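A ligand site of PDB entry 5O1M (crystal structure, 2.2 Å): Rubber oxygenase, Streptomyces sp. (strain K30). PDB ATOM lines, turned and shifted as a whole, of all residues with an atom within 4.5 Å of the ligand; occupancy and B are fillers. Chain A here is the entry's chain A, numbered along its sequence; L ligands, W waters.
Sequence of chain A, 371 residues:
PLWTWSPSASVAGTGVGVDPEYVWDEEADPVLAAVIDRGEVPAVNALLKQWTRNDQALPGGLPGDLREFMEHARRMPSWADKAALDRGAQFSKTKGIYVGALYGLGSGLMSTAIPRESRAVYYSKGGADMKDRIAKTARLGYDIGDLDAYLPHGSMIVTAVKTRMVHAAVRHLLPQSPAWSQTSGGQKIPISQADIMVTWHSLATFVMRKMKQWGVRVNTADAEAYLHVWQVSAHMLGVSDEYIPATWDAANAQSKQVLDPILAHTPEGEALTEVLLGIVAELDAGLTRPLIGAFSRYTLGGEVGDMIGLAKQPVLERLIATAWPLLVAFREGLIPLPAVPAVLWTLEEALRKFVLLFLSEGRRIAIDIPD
The backbone carbonyl oxygen (O) of Ala 128 sits at hydrogen-bond distance from the guanidinium group (NE) of Arg 133, at 2.8 Å. The backbone carbonyl oxygen (O) of Ser 124 sits at hydrogen-bond distance from the guanidinium group (NH1) of Arg 133 (3.4 Å). The backbone carbonyl oxygen of Val 121 sits at hydrogen-bond distance from the guanidinium group of Arg 133 (2.9 Å). The backbone carbonyl oxygen (O) of Asp 195 lies within hydrogen-bond range of the side-chain hydroxyl (OG1) of Thr 199, at 3.5 Å. NH1 of Arg 116 is in salt-bridge range of OD1 of Asp 195.
An iron atom (FE1) of the ligand is bound by a ring nitrogen (NE2) of His 167. The side-chain amino group (NZ) of Lys 136 binds an iron atom (FE1) of the ligand. The backbone NH (N) of Ala 128 sits at hydrogen-bond distance from an oxygen (O3) of the ligand, 2.8 Å away. OG of Ser 124 sits at hydrogen-bond distance from O4 of the ligand, 3.1 Å away. An oxygen (O4) of the ligand is in salt-bridge range of the guanidinium group of Arg 133 (3.3 Å).
Merely in contact with the ligand: Thr 199 (3.4 Å), Thr 163 (3.5 Å), Asp 195 (3.5 Å), Leu 140 (3.5 Å), Gly 127 (3.5 Å), Val 166 (3.6 Å), Arg 116 (3.6 Å), Ala 120 (3.6 Å), Glu 117 (3.7 Å), Ile 191 (3.7 Å), Val 170 (3.7 Å), Leu 237 (3.8 Å) and Ile 196 (3.8 Å). Hydrophobic or aromatic side chains that line the ligand: Ala 120, Ala 128, Leu 140, Val 166, His 167, Val 170, Ile 191, Ile 196 and Leu 237. Of the 24 residues printed, 18 come within 4 Å of the ligand. The nearest printed residue that does not touch the ligand is Trp 200 (4.1 Å).
Water W1 lies within hydrogen-bond range of N of Gly 127 (2.5 Å), O4 of the ligand (2.6 Å), O of Ser 124 (3.2 Å) and NE of Arg 133 (3.5 Å).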
ATOM      1  N   ARG A 116      10.961 -11.190  -8.214  1.00  0.00           N
ATOM      2  CA  ARG A 116      12.032 -10.482  -8.927  1.00  0.00           C
ATOM      3  C   ARG A 116      12.538  -9.289  -8.196  1.00  0.00           C
ATOM      4  O   ARG A 116      13.738  -9.009  -8.261  1.00  0.00           O
ATOM      5  CB  ARG A 116      11.616 -10.112 -10.321  1.00  0.00           C
ATOM      6  CG  ARG A 116      11.582 -11.353 -11.234  1.00  0.00           C
ATOM      7  CD  ARG A 116      10.780 -11.010 -12.477  1.00  0.00           C
ATOM      8  NE  ARG A 116      10.975 -11.952 -13.583  1.00  0.00           N
ATOM      9  CZ  ARG A 116      10.314 -11.859 -14.760  1.00  0.00           C
ATOM     10  NH1 ARG A 116       9.481 -10.845 -14.953  1.00  0.00           N
ATOM     11  NH2 ARG A 116      10.509 -12.741 -15.746  1.00  0.00           N
ATOM     12  N   GLU A 117      11.638  -8.587  -7.494  1.00  0.00           N
ATOM     13  CA  GLU A 117      12.003  -7.427  -6.699  1.00  0.00           C
ATOM     14  C   GLU A 117      12.842  -7.930  -5.524  1.00  0.00           C
ATOM     15  O   GLU A 117      13.879  -7.371  -5.224  1.00  0.00           O
ATOM     16  CB  GLU A 117      10.772  -6.691  -6.150  1.00  0.00           C
ATOM     17  CG  GLU A 117       9.934  -5.936  -7.121  1.00  0.00           C
ATOM     18  CD  GLU A 117       8.707  -5.195  -6.468  1.00  0.00           C
ATOM     19  OE1 GLU A 117       7.629  -5.121  -7.141  1.00  0.00           O
ATOM     20  OE2 GLU A 117       8.795  -4.599  -5.344  1.00  0.00           O
ATOM     21  N   ALA A 120      16.351  -9.099  -6.944  1.00  0.00           N
ATOM     22  CA  ALA A 120      17.134  -7.924  -7.357  1.00  0.00           C
ATOM     23  C   ALA A 120      17.630  -7.099  -6.150  1.00  0.00           C
ATOM     24  O   ALA A 120      18.775  -6.723  -6.079  1.00  0.00           O
ATOM     25  CB  ALA A 120      16.310  -7.058  -8.304  1.00  0.00           C
ATOM     26  N   VAL A 121      16.749  -6.844  -5.196  1.00  0.00           N
ATOM     27  CA  VAL A 121      17.086  -6.041  -4.037  1.00  0.00           C
ATOM     28  C   VAL A 121      18.115  -6.807  -3.196  1.00  0.00           C
ATOM     29  O   VAL A 121      19.085  -6.213  -2.706  1.00  0.00           O
ATOM     30  CB  VAL A 121      15.848  -5.664  -3.195  1.00  0.00           C
ATOM     31  CG1 VAL A 121      16.241  -5.104  -1.834  1.00  0.00           C
ATOM     32  CG2 VAL A 121      14.994  -4.671  -3.934  1.00  0.00           C
ATOM     33  N   SER A 124      21.504  -7.071  -5.028  1.00  0.00           N
ATOM     34  CA  SER A 124      22.061  -5.844  -5.591  1.00  0.00           C
ATOM     35  C   SER A 124      23.240  -5.391  -4.741  1.00  0.00           C
ATOM     36  O   SER A 124      23.158  -5.425  -3.521  1.00  0.00           O
ATOM     37  CB  SER A 124      20.991  -4.736  -5.690  1.00  0.00           C
ATOM     38  OG  SER A 124      21.536  -3.583  -6.304  1.00  0.00           O
ATOM     39  N   GLY A 127      24.930  -0.393  -3.917  1.00  0.00           N
ATOM     40  CA  GLY A 127      23.884   0.632  -3.855  1.00  0.00           C
ATOM     41  C   GLY A 127      23.693   1.076  -2.432  1.00  0.00           C
ATOM     42  O   GLY A 127      24.649   1.144  -1.679  1.00  0.00           O
ATOM     43  N   ALA A 128      22.445   1.339  -2.075  1.00  0.00           N
ATOM     44  CA  ALA A 128      22.088   1.736  -0.726  1.00  0.00           C
ATOM     45  C   ALA A 128      22.297   0.565   0.220  1.00  0.00           C
ATOM     46  O   ALA A 128      22.304  -0.590  -0.206  1.00  0.00           O
ATOM     47  CB  ALA A 128      20.645   2.190  -0.676  1.00  0.00           C
ATOM     48  N   ARG A 133      17.514   0.211   1.309  1.00  0.00           N
ATOM     49  CA  ARG A 133      16.984  -0.568   0.151  1.00  0.00           C
ATOM     50  C   ARG A 133      15.567  -1.146   0.351  1.00  0.00           C
ATOM     51  O   ARG A 133      14.760  -1.176  -0.587  1.00  0.00           O
ATOM     52  CB  ARG A 133      17.888  -1.774  -0.159  1.00  0.00           C
ATOM     53  CG  ARG A 133      18.587  -1.693  -1.496  1.00  0.00           C
ATOM     54  CD  ARG A 133      19.467  -2.901  -1.691  1.00  0.00           C
ATOM     55  NE  ARG A 133      20.736  -2.825  -0.997  1.00  0.00           N
ATOM     56  CZ  ARG A 133      21.473  -3.880  -0.615  1.00  0.00           C
ATOM     57  NH1 ARG A 133      21.106  -5.139  -0.863  1.00  0.00           N
ATOM     58  NH2 ARG A 133      22.609  -3.657   0.023  1.00  0.00           N
ATOM     59  N   LYS A 136      12.529   1.259   0.032  1.00  0.00           N
ATOM     60  CA  LYS A 136      12.662   2.184  -1.081  1.00  0.00           C
ATOM     61  C   LYS A 136      11.316   2.479  -1.836  1.00  0.00           C
ATOM     62  O   LYS A 136      11.131   3.595  -2.283  1.00  0.00           O
ATOM     63  CB  LYS A 136      13.689   1.707  -2.091  1.00  0.00           C
ATOM     64  CG  LYS A 136      13.193   0.567  -2.949  1.00  0.00           C
ATOM     65  CD  LYS A 136      14.325  -0.104  -3.717  1.00  0.00           C
ATOM     66  CE  LYS A 136      13.797  -1.255  -4.551  1.00  0.00           C
ATOM     67  NZ  LYS A 136      12.801  -0.883  -5.611  1.00  0.00           N
ATOM     68  N   THR A 137      10.448   1.482  -1.993  1.00  0.00           N
ATOM     69  CA  THR A 137       9.172   1.685  -2.697  1.00  0.00           C
ATOM     70  C   THR A 137       8.201   2.519  -1.869  1.00  0.00           C
ATOM     71  O   THR A 137       7.511   3.407  -2.417  1.00  0.00           O
ATOM     72  CB  THR A 137       8.506   0.371  -3.185  1.00  0.00           C
ATOM     73  OG1 THR A 137       8.029  -0.435  -2.073  1.00  0.00           O
ATOM     74  CG2 THR A 137       9.522  -0.408  -4.058  1.00  0.00           C
ATOM     75  N   LEU A 140       9.565   6.089  -1.597  1.00  0.00           N
ATOM     76  CA  LEU A 140       9.177   6.755  -2.834  1.00  0.00           C
ATOM     77  C   LEU A 140       7.630   6.931  -3.002  1.00  0.00           C
ATOM     78  O   LEU A 140       7.172   8.005  -3.410  1.00  0.00           O
ATOM     79  CB  LEU A 140       9.797   6.098  -4.084  1.00  0.00           C
ATOM     80  CG  LEU A 140       9.789   7.073  -5.270  1.00  0.00           C
ATOM     81  CD1 LEU A 140      11.067   6.978  -6.096  1.00  0.00           C
ATOM     82  CD2 LEU A 140       8.585   6.772  -6.152  1.00  0.00           C
ATOM     83  N   THR A 163      16.034   7.837  -9.770  1.00  0.00           N
ATOM     84  CA  THR A 163      15.546   6.456  -9.629  1.00  0.00           C
ATOM     85  C   THR A 163      15.633   5.692 -10.954  1.00  0.00           C
ATOM     86  O   THR A 163      16.083   4.550 -11.015  1.00  0.00           O
ATOM     87  CB  THR A 163      14.115   6.412  -9.073  1.00  0.00           C
ATOM     88  OG1 THR A 163      14.072   7.043  -7.790  1.00  0.00           O
ATOM     89  CG2 THR A 163      13.656   4.990  -8.927  1.00  0.00           C
ATOM     90  N   VAL A 166      19.132   4.783 -11.570  1.00  0.00           N
ATOM     91  CA  VAL A 166      19.538   3.648 -10.730  1.00  0.00           C
ATOM     92  C   VAL A 166      19.065   2.298 -11.324  1.00  0.00           C
ATOM     93  O   VAL A 166      19.851   1.316 -11.396  1.00  0.00           O
ATOM     94  CB  VAL A 166      19.072   3.844  -9.317  1.00  0.00           C
ATOM     95  CG1 VAL A 166      19.268   2.568  -8.471  1.00  0.00           C
ATOM     96  CG2 VAL A 166      19.817   5.026  -8.670  1.00  0.00           C
ATOM     97  N   HIS A 167      17.819   2.252 -11.806  1.00  0.00           N
ATOM     98  CA  HIS A 167      17.295   1.051 -12.444  1.00  0.00           C
ATOM     99  C   HIS A 167      18.077   0.728 -13.696  1.00  0.00           C
ATOM    100  O   HIS A 167      18.404  -0.427 -13.915  1.00  0.00           O
ATOM    101  CB  HIS A 167      15.806   1.219 -12.780  1.00  0.00           C
ATOM    102  CG  HIS A 167      14.920   1.201 -11.577  1.00  0.00           C
ATOM    103  ND1 HIS A 167      13.663   1.773 -11.565  1.00  0.00           N
ATOM    104  CD2 HIS A 167      15.086   0.659 -10.341  1.00  0.00           C
ATOM    105  CE1 HIS A 167      13.108   1.582 -10.383  1.00  0.00           C
ATOM    106  NE2 HIS A 167      13.954   0.911  -9.618  1.00  0.00           N
ATOM    107  N   VAL A 170      21.378  -0.835 -12.623  1.00  0.00           N
ATOM    108  CA  VAL A 170      21.183  -2.188 -12.119  1.00  0.00           C
ATOM    109  C   VAL A 170      21.028  -3.197 -13.285  1.00  0.00           C
ATOM    110  O   VAL A 170      21.448  -4.340 -13.154  1.00  0.00           O
ATOM    111  CB  VAL A 170      19.935  -2.289 -11.141  1.00  0.00           C
ATOM    112  CG1 VAL A 170      19.631  -3.724 -10.717  1.00  0.00           C
ATOM    113  CG2 VAL A 170      20.142  -1.456  -9.886  1.00  0.00           C
ATOM    114  N   ILE A 191      14.559  -5.888 -14.312  1.00  0.00           N
ATOM    115  CA  ILE A 191      13.675  -4.728 -14.259  1.00  0.00           C
ATOM    116  C   ILE A 191      13.032  -4.364 -15.571  1.00  0.00           C
ATOM    117  O   ILE A 191      13.235  -3.241 -16.081  1.00  0.00           O
ATOM    118  CB  ILE A 191      14.330  -3.497 -13.597  1.00  0.00           C
ATOM    119  CG1 ILE A 191      15.243  -3.916 -12.448  1.00  0.00           C
ATOM    120  CG2 ILE A 191      13.229  -2.574 -13.053  1.00  0.00           C
ATOM    121  CD1 ILE A 191      15.903  -2.701 -11.828  1.00  0.00           C
ATOM    122  N   ASP A 195       7.809  -5.528 -14.985  1.00  0.00           N
ATOM    123  CA  ASP A 195       8.214  -5.625 -13.557  1.00  0.00           C
ATOM    124  C   ASP A 195       7.907  -4.352 -12.825  1.00  0.00           C
ATOM    125  O   ASP A 195       7.338  -4.400 -11.752  1.00  0.00           O
ATOM    126  CB  ASP A 195       9.707  -5.930 -13.355  1.00  0.00           C
ATOM    127  CG  ASP A 195      10.127  -7.320 -13.855  1.00  0.00           C
ATOM    128  OD1 ASP A 195       9.430  -8.322 -13.601  1.00  0.00           O
ATOM    129  OD2 ASP A 195      11.214  -7.400 -14.455  1.00  0.00           O
ATOM    130  N   ILE A 196       8.247  -3.217 -13.439  1.00  0.00           N
ATOM    131  CA  ILE A 196       7.930  -1.937 -12.865  1.00  0.00           C
ATOM    132  C   ILE A 196       6.387  -1.762 -12.617  1.00  0.00           C
ATOM    133  O   ILE A 196       5.959  -1.249 -11.578  1.00  0.00           O
ATOM    134  CB  ILE A 196       8.470  -0.761 -13.747  1.00  0.00           C
ATOM    135  CG1 ILE A 196       9.978  -0.793 -13.861  1.00  0.00           C
ATOM    136  CG2 ILE A 196       8.052   0.620 -13.139  1.00  0.00           C
ATOM    137  CD1 ILE A 196      10.556   0.270 -14.796  1.00  0.00           C
ATOM    138  N   THR A 199       5.168  -3.519  -9.554  1.00  0.00           N
ATOM    139  CA  THR A 199       5.408  -2.735  -8.326  1.00  0.00           C
ATOM    140  C   THR A 199       4.409  -1.607  -8.175  1.00  0.00           C
ATOM    141  O   THR A 199       3.931  -1.318  -7.090  1.00  0.00           O
ATOM    142  CB  THR A 199       6.846  -2.187  -8.316  1.00  0.00           C
ATOM    143  OG1 THR A 199       7.733  -3.277  -8.464  1.00  0.00           O
ATOM    144  CG2 THR A 199       7.199  -1.448  -6.984  1.00  0.00           C
ATOM    145  N   TRP A 200       4.101  -0.974  -9.308  1.00  0.00           N
ATOM    146  CA  TRP A 200       3.095   0.043  -9.397  1.00  0.00           C
ATOM    147  C   TRP A 200       1.755  -0.436  -8.874  1.00  0.00           C
ATOM    148  O   TRP A 200       1.098   0.317  -8.146  1.00  0.00           O
ATOM    149  CB  TRP A 200       2.961   0.543 -10.854  1.00  0.00           C
ATOM    150  CG  TRP A 200       2.256   1.813 -11.070  1.00  0.00           C
ATOM    151  CD1 TRP A 200       2.831   3.054 -11.161  1.00  0.00           C
ATOM    152  CD2 TRP A 200       0.830   2.016 -11.241  1.00  0.00           C
ATOM    153  NE1 TRP A 200       1.875   4.007 -11.378  1.00  0.00           N
ATOM    154  CE2 TRP A 200       0.638   3.400 -11.451  1.00  0.00           C
ATOM    155  CE3 TRP A 200      -0.275   1.195 -11.186  1.00  0.00           C
ATOM    156  CZ2 TRP A 200      -0.626   3.977 -11.683  1.00  0.00           C
ATOM    157  CZ3 TRP A 200      -1.553   1.768 -11.455  1.00  0.00           C
ATOM    158  CH2 TRP A 200      -1.711   3.150 -11.677  1.00  0.00           C
ATOM    159  N   LEU A 203       1.662  -0.644  -5.226  1.00  0.00           N
ATOM    160  CA  LEU A 203       1.551   0.677  -4.613  1.00  0.00           C
ATOM    161  C   LEU A 203       0.151   1.317  -4.889  1.00  0.00           C
ATOM    162  O   LEU A 203      -0.748   1.130  -4.109  1.00  0.00           O
ATOM    163  CB  LEU A 203       2.665   1.564  -5.075  1.00  0.00           C
ATOM    164  CG  LEU A 203       4.043   1.113  -4.568  1.00  0.00           C
ATOM    165  CD1 LEU A 203       5.165   1.648  -5.480  1.00  0.00           C
ATOM    166  CD2 LEU A 203       4.317   1.593  -3.132  1.00  0.00           C
ATOM    167  N   LEU A 237       9.158   7.884 -13.970  1.00  0.00           N
ATOM    168  CA  LEU A 237      10.043   6.758 -13.739  1.00  0.00           C
ATOM    169  C   LEU A 237      10.585   6.050 -14.955  1.00  0.00           C
ATOM    170  O   LEU A 237      11.502   5.242 -14.785  1.00  0.00           O
ATOM    171  CB  LEU A 237       9.395   5.720 -12.782  1.00  0.00           C
ATOM    172  CG  LEU A 237       9.224   6.187 -11.338  1.00  0.00           C
ATOM    173  CD1 LEU A 237       8.276   5.277 -10.558  1.00  0.00           C
ATOM    174  CD2 LEU A 237      10.563   6.342 -10.657  1.00  0.00           C
ATOM    175  N   ILE A 367      19.819   9.713  -3.578  1.00  0.00           N
ATOM    176  CA  ILE A 367      19.747   8.578  -4.480  1.00  0.00           C
ATOM    177  C   ILE A 367      20.983   8.594  -5.380  1.00  0.00           C
ATOM    178  O   ILE A 367      21.209   9.531  -6.142  1.00  0.00           O
ATOM    179  CB  ILE A 367      18.424   8.668  -5.283  1.00  0.00           C
ATOM    180  CG1 ILE A 367      17.272   8.483  -4.296  1.00  0.00           C
ATOM    181  CG2 ILE A 367      18.365   7.604  -6.369  1.00  0.00           C
ATOM    182  CD1 ILE A 367      15.895   8.810  -4.841  1.00  0.00           C
ATOM    183  N   ASP A 368      21.799   7.551  -5.241  1.00  0.00           N
ATOM    184  CA  ASP A 368      23.137   7.459  -5.833  1.00  0.00           C
ATOM    185  C   ASP A 368      23.178   6.373  -6.899  1.00  0.00           C
ATOM    186  O   ASP A 368      22.551   5.352  -6.743  1.00  0.00           O
ATOM    187  CB  ASP A 368      24.178   7.077  -4.745  1.00  0.00           C
ATOM    188  CG  ASP A 368      24.632   8.272  -3.868  1.00  0.00           C
ATOM    189  OD1 ASP A 368      24.773   9.405  -4.389  1.00  0.00           O
ATOM    190  OD2 ASP A 368      24.873   8.081  -2.637  1.00  0.00           O
HETATM  191  C1  LIG L   1      16.532   1.275  -6.593  1.00  0.00           C
HETATM  192  C2  LIG L   1      11.981   2.800  -6.481  1.00  0.00           C
HETATM  193  C3  LIG L   1      10.743  -0.891  -9.303  1.00  0.00           C
HETATM  194  C4  LIG L   1      14.836  -2.954  -8.149  1.00  0.00           C
HETATM  195  C5  LIG L   1      15.395   2.056  -6.403  1.00  0.00           C
HETATM  196  C6  LIG L   1      15.411   3.271  -5.715  1.00  0.00           C
HETATM  197  C7  LIG L   1      14.150   3.732  -5.678  1.00  0.00           C
HETATM  198  C8  LIG L   1      13.346   2.758  -6.297  1.00  0.00           C
HETATM  199  C9  LIG L   1      13.687   4.996  -4.997  1.00  0.00           C
HETATM  200  C10 LIG L   1      16.613   3.975  -5.139  1.00  0.00           C
HETATM  201  C11 LIG L   1      17.023   3.435  -3.722  1.00  0.00           C
HETATM  202  C12 LIG L   1      18.533   3.421  -3.893  1.00  0.00           C
HETATM  203  O1  LIG L   1      19.170   4.424  -3.410  1.00  0.00           O
HETATM  204  O2  LIG L   1      19.157   2.504  -4.589  1.00  0.00           O
HETATM  205  C13 LIG L   1      11.244   1.931  -7.287  1.00  0.00           C
HETATM  206  C14 LIG L   1       9.878   2.152  -7.642  1.00  0.00           C
HETATM  207  C15 LIG L   1       9.470   1.144  -8.451  1.00  0.00           C
HETATM  208  C16 LIG L   1      10.698   0.282  -8.556  1.00  0.00           C
HETATM  209  C17 LIG L   1       9.023   3.268  -7.177  1.00  0.00           C
HETATM  210  C18 LIG L   1       8.187   0.898  -9.173  1.00  0.00           C
HETATM  211  C19 LIG L   1       7.055   1.899  -9.429  1.00  0.00           C
HETATM  212  C20 LIG L   1      11.721  -1.804  -9.238  1.00  0.00           C
HETATM  213  C21 LIG L   1      11.651  -3.143  -9.710  1.00  0.00           C
HETATM  214  C22 LIG L   1      12.808  -3.742  -9.320  1.00  0.00           C
HETATM  215  C23 LIG L   1      13.581  -2.745  -8.649  1.00  0.00           C
HETATM  216  C24 LIG L   1      10.480  -3.779 -10.433  1.00  0.00           C
HETATM  217  C25 LIG L   1      13.266  -5.135  -9.534  1.00  0.00           C
HETATM  218  C26 LIG L   1      12.572  -6.270 -10.227  1.00  0.00           C
HETATM  219  C27 LIG L   1      15.678  -1.958  -7.642  1.00  0.00           C
HETATM  220  C28 LIG L   1      17.120  -2.162  -7.349  1.00  0.00           C
HETATM  221  C29 LIG L   1      17.592  -0.985  -6.924  1.00  0.00           C
HETATM  222  C30 LIG L   1      16.458  -0.036  -7.003  1.00  0.00           C
HETATM  223  C31 LIG L   1      17.859  -3.467  -7.428  1.00  0.00           C
HETATM  224  C32 LIG L   1      18.974  -0.740  -6.419  1.00  0.00           C
HETATM  225  C33 LIG L   1      18.938  -1.156  -4.966  1.00  0.00           C
HETATM  226  C34 LIG L   1      20.190  -0.695  -4.228  1.00  0.00           C
HETATM  227  O3  LIG L   1      20.370   0.488  -3.766  1.00  0.00           O
HETATM  228  O4  LIG L   1      21.110  -1.553  -4.011  1.00  0.00           O
HETATM  229  N1  LIG L   1      14.102   1.763  -6.689  1.00  0.00           N
HETATM  230  N2  LIG L   1      11.686   0.844  -7.865  1.00  0.00           N
HETATM  231  N3  LIG L   1      12.848  -1.589  -8.574  1.00  0.00           N
HETATM  232  N4  LIG L   1      15.363  -0.689  -7.431  1.00  0.00           N
HETATM  233 FE1  LIG L   1      13.483   0.092  -7.694  1.00  0.00          FE
HETATM  234  O   HOH W   1      23.473  -2.310  -3.100  1.00  0.00           O
